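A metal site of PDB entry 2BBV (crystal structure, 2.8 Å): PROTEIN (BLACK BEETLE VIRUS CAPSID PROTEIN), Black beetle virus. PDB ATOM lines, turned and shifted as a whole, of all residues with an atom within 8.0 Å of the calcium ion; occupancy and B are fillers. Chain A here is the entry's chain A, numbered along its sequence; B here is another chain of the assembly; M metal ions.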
ATOM      1  N   THR A 216      -5.854 -19.825  21.677  1.00  0.00           N
ATOM      2  CA  THR A 216      -4.670 -19.255  22.325  1.00  0.00           C
ATOM      3  C   THR A 216      -5.047 -18.317  23.442  1.00  0.00           C
ATOM      4  O   THR A 216      -6.025 -17.564  23.352  1.00  0.00           O
ATOM      5  CB  THR A 216      -3.773 -18.527  21.249  1.00  0.00           C
ATOM      6  OG1 THR A 216      -2.425 -18.550  21.820  1.00  0.00           O
ATOM      7  CG2 THR A 216      -4.265 -17.124  20.933  1.00  0.00           C
ATOM      8  N   LEU A 217      -4.274 -18.407  24.505  1.00  0.00           N
ATOM      9  CA  LEU A 217      -4.462 -17.573  25.700  1.00  0.00           C
ATOM     10  C   LEU A 217      -3.700 -16.274  25.453  1.00  0.00           C
ATOM     11  O   LEU A 217      -2.497 -16.414  25.093  1.00  0.00           O
ATOM     12  CB  LEU A 217      -3.926 -18.402  26.852  1.00  0.00           C
ATOM     13  CG  LEU A 217      -4.812 -19.097  27.856  1.00  0.00           C
ATOM     14  CD1 LEU A 217      -6.284 -19.100  27.500  1.00  0.00           C
ATOM     15  CD2 LEU A 217      -4.316 -20.541  27.983  1.00  0.00           C
ATOM     16  N   VAL A 218      -4.338 -15.125  25.614  1.00  0.00           N
ATOM     17  CA  VAL A 218      -3.632 -13.827  25.425  1.00  0.00           C
ATOM     18  C   VAL A 218      -3.575 -13.135  26.800  1.00  0.00           C
ATOM     19  O   VAL A 218      -4.614 -13.078  27.472  1.00  0.00           O
ATOM     20  CB  VAL A 218      -4.282 -12.985  24.346  1.00  0.00           C
ATOM     21  CG1 VAL A 218      -4.141 -13.514  22.948  1.00  0.00           C
ATOM     22  CG2 VAL A 218      -5.746 -12.742  24.685  1.00  0.00           C
ATOM     23  N   GLY A 219      -2.393 -12.712  27.209  1.00  0.00           N
ATOM     24  CA  GLY A 219      -2.281 -12.052  28.508  1.00  0.00           C
ATOM     25  C   GLY A 219      -1.589 -12.864  29.577  1.00  0.00           C
ATOM     26  O   GLY A 219      -1.565 -12.436  30.771  1.00  0.00           O
ATOM     27  N   LEU A 220      -1.024 -13.985  29.205  1.00  0.00           N
ATOM     28  CA  LEU A 220      -0.285 -14.860  30.126  1.00  0.00           C
ATOM     29  C   LEU A 220       1.129 -14.337  30.372  1.00  0.00           C
ATOM     30  O   LEU A 220       1.872 -14.884  31.206  1.00  0.00           O
ATOM     31  CB  LEU A 220      -0.279 -16.250  29.460  1.00  0.00           C
ATOM     32  CG  LEU A 220      -0.883 -17.383  30.257  1.00  0.00           C
ATOM     33  CD1 LEU A 220      -2.045 -16.852  31.114  1.00  0.00           C
ATOM     34  CD2 LEU A 220      -1.386 -18.426  29.291  1.00  0.00           C
ATOM     35  N   ASP A 221       1.512 -13.309  29.634  1.00  0.00           N
ATOM     36  CA  ASP A 221       2.873 -12.720  29.746  1.00  0.00           C
ATOM     37  C   ASP A 221       2.933 -11.885  31.036  1.00  0.00           C
ATOM     38  O   ASP A 221       3.983 -11.389  31.457  1.00  0.00           O
ATOM     39  CB  ASP A 221       3.187 -11.920  28.486  1.00  0.00           C
ATOM     40  CG  ASP A 221       3.771 -12.752  27.354  1.00  0.00           C
ATOM     41  OD1 ASP A 221       4.759 -13.489  27.559  1.00  0.00           O
ATOM     42  OD2 ASP A 221       3.233 -12.670  26.214  1.00  0.00           O
ATOM     43  N   GLY A 222       1.758 -11.759  31.615  1.00  0.00           N
ATOM     44  CA  GLY A 222       1.524 -11.013  32.835  1.00  0.00           C
ATOM     45  C   GLY A 222       2.001 -11.839  34.013  1.00  0.00           C
ATOM     46  O   GLY A 222       2.274 -11.268  35.088  1.00  0.00           O
ATOM     47  N   LEU A 224       4.747 -13.287  34.163  1.00  0.00           N
ATOM     48  CA  LEU A 224       6.190 -13.136  34.097  1.00  0.00           C
ATOM     49  C   LEU A 224       6.820 -12.050  34.909  1.00  0.00           C
ATOM     50  O   LEU A 224       8.083 -11.906  34.860  1.00  0.00           O
ATOM     51  CB  LEU A 224       6.520 -13.027  32.586  1.00  0.00           C
ATOM     52  CG  LEU A 224       6.138 -14.282  31.804  1.00  0.00           C
ATOM     53  CD1 LEU A 224       6.589 -14.231  30.375  1.00  0.00           C
ATOM     54  CD2 LEU A 224       6.746 -15.461  32.540  1.00  0.00           C
ATOM     55  N   VAL A 269       4.795 -24.041  21.320  1.00  0.00           N
ATOM     56  CA  VAL A 269       4.521 -22.959  22.243  1.00  0.00           C
ATOM     57  C   VAL A 269       4.876 -21.637  21.551  1.00  0.00           C
ATOM     58  O   VAL A 269       4.335 -20.575  21.886  1.00  0.00           O
ATOM     59  CB  VAL A 269       5.361 -23.118  23.502  1.00  0.00           C
ATOM     60  CG1 VAL A 269       5.730 -21.778  24.152  1.00  0.00           C
ATOM     61  CG2 VAL A 269       4.657 -23.933  24.598  1.00  0.00           C
ATOM     62  N   ALA A 270       5.785 -21.738  20.595  1.00  0.00           N
ATOM     63  CA  ALA A 270       6.295 -20.556  19.865  1.00  0.00           C
ATOM     64  C   ALA A 270       5.290 -20.003  18.850  1.00  0.00           C
ATOM     65  O   ALA A 270       5.223 -18.799  18.592  1.00  0.00           O
ATOM     66  CB  ALA A 270       7.578 -20.899  19.109  1.00  0.00           C
ATOM     67  N   SER A 272       1.992 -20.415  19.110  1.00  0.00           N
ATOM     68  CA  SER A 272       0.812 -20.038  19.903  1.00  0.00           C
ATOM     69  C   SER A 272       0.972 -18.612  20.412  1.00  0.00           C
ATOM     70  O   SER A 272      -0.002 -17.856  20.571  1.00  0.00           O
ATOM     71  CB  SER A 272       0.659 -20.967  21.099  1.00  0.00           C
ATOM     72  OG  SER A 272       1.595 -20.601  22.117  1.00  0.00           O
ATOM     73  N   GLY A 273       2.218 -18.272  20.659  1.00  0.00           N
ATOM     74  CA  GLY A 273       2.588 -16.961  21.184  1.00  0.00           C
ATOM     75  C   GLY A 273       2.356 -16.908  22.698  1.00  0.00           C
ATOM     76  O   GLY A 273       2.246 -15.825  23.280  1.00  0.00           O
ATOM     77  N   GLN A 274       2.277 -18.087  23.303  1.00  0.00           N
ATOM     78  CA  GLN A 274       2.093 -18.227  24.764  1.00  0.00           C
ATOM     79  C   GLN A 274       3.442 -18.398  25.453  1.00  0.00           C
ATOM     80  O   GLN A 274       4.334 -19.110  24.948  1.00  0.00           O
ATOM     81  CB  GLN A 274       1.248 -19.457  25.088  1.00  0.00           C
ATOM     82  CG  GLN A 274      -0.230 -19.266  24.734  1.00  0.00           C
ATOM     83  CD  GLN A 274      -1.131 -20.369  25.294  1.00  0.00           C
ATOM     84  OE1 GLN A 274      -0.853 -20.907  26.360  1.00  0.00           O
ATOM     85  NE2 GLN A 274      -2.209 -20.738  24.627  1.00  0.00           N
ATOM     86  N   PRO A 275       3.654 -17.760  26.614  1.00  0.00           N
ATOM     87  CA  PRO A 275       4.904 -17.849  27.343  1.00  0.00           C
ATOM     88  C   PRO A 275       5.100 -19.238  27.881  1.00  0.00           C
ATOM     89  O   PRO A 275       6.264 -19.649  28.130  1.00  0.00           O
ATOM     90  CB  PRO A 275       4.754 -16.933  28.516  1.00  0.00           C
ATOM     91  CG  PRO A 275       3.345 -16.380  28.482  1.00  0.00           C
ATOM     92  CD  PRO A 275       2.654 -16.911  27.258  1.00  0.00           C
ATOM     93  N   PHE A 276       3.988 -19.931  28.109  1.00  0.00           N
ATOM     94  CA  PHE A 276       4.082 -21.299  28.619  1.00  0.00           C
ATOM     95  C   PHE A 276       2.882 -22.156  28.193  1.00  0.00           C
ATOM     96  O   PHE A 276       2.132 -21.781  27.273  1.00  0.00           O
ATOM     97  CB  PHE A 276       4.256 -21.337  30.149  1.00  0.00           C
ATOM     98  CG  PHE A 276       3.511 -20.255  30.914  1.00  0.00           C
ATOM     99  CD1 PHE A 276       4.120 -19.020  31.168  1.00  0.00           C
ATOM    100  CD2 PHE A 276       2.224 -20.512  31.399  1.00  0.00           C
ATOM    101  CE1 PHE A 276       3.437 -18.041  31.900  1.00  0.00           C
ATOM    102  CE2 PHE A 276       1.547 -19.540  32.125  1.00  0.00           C
ATOM    103  CZ  PHE A 276       2.145 -18.298  32.376  1.00  0.00           C
ATOM    104  N   ALA B 157       3.247 -13.210  16.270  1.00  0.00           N
ATOM    105  CA  ALA B 157       2.574 -13.809  17.444  1.00  0.00           C
ATOM    106  C   ALA B 157       2.965 -13.139  18.737  1.00  0.00           C
ATOM    107  O   ALA B 157       2.933 -13.793  19.811  1.00  0.00           O
ATOM    108  CB  ALA B 157       2.713 -15.305  17.415  1.00  0.00           C
ATOM    109  N   SER B 158       3.292 -11.851  18.701  1.00  0.00           N
ATOM    110  CA  SER B 158       3.651 -11.154  19.959  1.00  0.00           C
ATOM    111  C   SER B 158       2.722  -9.962  20.166  1.00  0.00           C
ATOM    112  O   SER B 158       3.139  -8.973  20.808  1.00  0.00           O
ATOM    113  CB  SER B 158       5.080 -10.652  19.941  1.00  0.00           C
ATOM    114  OG  SER B 158       6.003 -11.670  19.637  1.00  0.00           O
ATOM    115  N   ARG B 159       1.525 -10.093  19.591  1.00  0.00           N
ATOM    116  CA  ARG B 159       0.573  -8.986  19.655  1.00  0.00           C
ATOM    117  C   ARG B 159       0.132  -8.637  21.054  1.00  0.00           C
ATOM    118  O   ARG B 159      -0.044  -7.421  21.355  1.00  0.00           O
ATOM    119  CB  ARG B 159      -0.574  -9.169  18.694  1.00  0.00           C
ATOM    120  CG  ARG B 159      -0.230  -8.871  17.256  1.00  0.00           C
ATOM    121  CD  ARG B 159       1.133  -8.297  17.017  1.00  0.00           C
ATOM    122  NE  ARG B 159       1.428  -8.228  15.581  1.00  0.00           N
ATOM    123  CZ  ARG B 159       2.583  -7.771  15.082  1.00  0.00           C
ATOM    124  NH1 ARG B 159       3.528  -7.295  15.899  1.00  0.00           N
ATOM    125  NH2 ARG B 159       2.847  -7.742  13.765  1.00  0.00           N
ATOM    126  N   SER B 160       0.008  -9.616  21.937  1.00  0.00           N
ATOM    127  CA  SER B 160      -0.447  -9.362  23.303  1.00  0.00           C
ATOM    128  C   SER B 160       0.589  -9.354  24.386  1.00  0.00           C
ATOM    129  O   SER B 160       0.215  -9.711  25.535  1.00  0.00           O
ATOM    130  CB  SER B 160      -1.564 -10.322  23.678  1.00  0.00           C
ATOM    131  OG  SER B 160      -1.494 -11.512  22.923  1.00  0.00           O
ATOM    132  N   ASP B 161       1.810  -8.976  24.095  1.00  0.00           N
ATOM    133  CA  ASP B 161       2.846  -8.967  25.178  1.00  0.00           C
ATOM    134  C   ASP B 161       2.512  -7.857  26.155  1.00  0.00           C
ATOM    135  O   ASP B 161       2.448  -8.154  27.371  1.00  0.00           O
ATOM    136  CB  ASP B 161       4.240  -8.977  24.603  1.00  0.00           C
ATOM    137  CG  ASP B 161       4.695 -10.323  24.092  1.00  0.00           C
ATOM    138  OD1 ASP B 161       3.848 -11.258  24.015  1.00  0.00           O
ATOM    139  OD2 ASP B 161       5.866 -10.542  23.738  1.00  0.00           O
ATOM    140  N   GLN B 162       2.255  -6.660  25.657  1.00  0.00           N
ATOM    141  CA  GLN B 162       1.925  -5.470  26.407  1.00  0.00           C
ATOM    142  C   GLN B 162       0.473  -5.415  26.932  1.00  0.00           C
ATOM    143  O   GLN B 162       0.197  -5.130  28.120  1.00  0.00           O
ATOM    144  CB  GLN B 162       2.112  -4.177  25.612  1.00  0.00           C
ATOM    145  CG  GLN B 162       3.514  -3.752  25.228  1.00  0.00           C
ATOM    146  CD  GLN B 162       4.485  -4.117  26.321  1.00  0.00           C
ATOM    147  OE1 GLN B 162       4.531  -3.477  27.360  1.00  0.00           O
ATOM    148  NE2 GLN B 162       5.230  -5.173  26.062  1.00  0.00           N
ATOM    149  N   GLU B 257      -3.804 -12.941  17.353  1.00  0.00           N
ATOM    150  CA  GLU B 257      -2.419 -13.286  17.034  1.00  0.00           C
ATOM    151  C   GLU B 257      -2.224 -13.891  15.660  1.00  0.00           C
ATOM    152  O   GLU B 257      -3.049 -14.731  15.252  1.00  0.00           O
ATOM    153  CB  GLU B 257      -1.941 -14.314  18.092  1.00  0.00           C
ATOM    154  CG  GLU B 257      -1.875 -13.653  19.479  1.00  0.00           C
ATOM    155  CD  GLU B 257      -0.675 -12.767  19.637  1.00  0.00           C
ATOM    156  OE1 GLU B 257      -0.079 -12.564  18.572  1.00  0.00           O
ATOM    157  OE2 GLU B 257      -0.289 -12.309  20.692  1.00  0.00           O
ATOM    158  N   ASN B 324      -1.214  -5.444  30.689  1.00  0.00           N
ATOM    159  CA  ASN B 324      -0.633  -6.674  31.253  1.00  0.00           C
ATOM    160  C   ASN B 324       0.348  -6.200  32.346  1.00  0.00           C
ATOM    161  O   ASN B 324       1.147  -5.301  32.040  1.00  0.00           O
ATOM    162  CB  ASN B 324       0.129  -7.447  30.175  1.00  0.00           C
ATOM    163  CG  ASN B 324      -0.776  -8.351  29.341  1.00  0.00           C
ATOM    164  OD1 ASN B 324      -0.703  -8.325  28.107  1.00  0.00           O
ATOM    165  ND2 ASN B 324      -1.630  -9.160  29.935  1.00  0.00           N
ATOM    166  N   ASN B 326       2.989  -7.207  33.331  1.00  0.00           N
ATOM    167  CA  ASN B 326       4.381  -7.294  32.921  1.00  0.00           C
ATOM    168  C   ASN B 326       4.786  -6.134  31.990  1.00  0.00           C
ATOM    169  O   ASN B 326       6.003  -5.869  31.908  1.00  0.00           O
ATOM    170  CB  ASN B 326       4.640  -8.593  32.148  1.00  0.00           C
ATOM    171  CG  ASN B 326       3.849  -8.599  30.841  1.00  0.00           C
ATOM    172  OD1 ASN B 326       4.406  -8.563  29.748  1.00  0.00           O
ATOM    173  ND2 ASN B 326       2.520  -8.643  30.985  1.00  0.00           N
HETATM  174 CA    CA M   1       2.837 -13.764  24.098  1.00  0.00          CA
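O of Gly 273 binds the calcium ion, at 2.3 Å. The calcium ion is bound by the side-chain carboxylate (OD2) of Asp 221, at 2.4 Å. The side-chain carboxylate (OD1) of Asp 161 of chain B binds the calcium ion (2.7 Å). The calcium ion has three donor atoms within binding distance.
Of the 24 residues printed, 3 come within 4 Å of the calcium ion.
The backbone carbonyl oxygen (O) of Asp 221 lies close to the side-chain amide nitrogen (ND2) of Asn 326 of chain B, 3.1 Å away. O of Asp 161 of chain B sits close to OD1 of Asn 324 of chain B. The backbone carbonyl oxygen (O) of Asp 161 of chain B sits close to the side-chain amide oxygen (OD1) of Asn 326 of chain B, at 3.1 Å.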
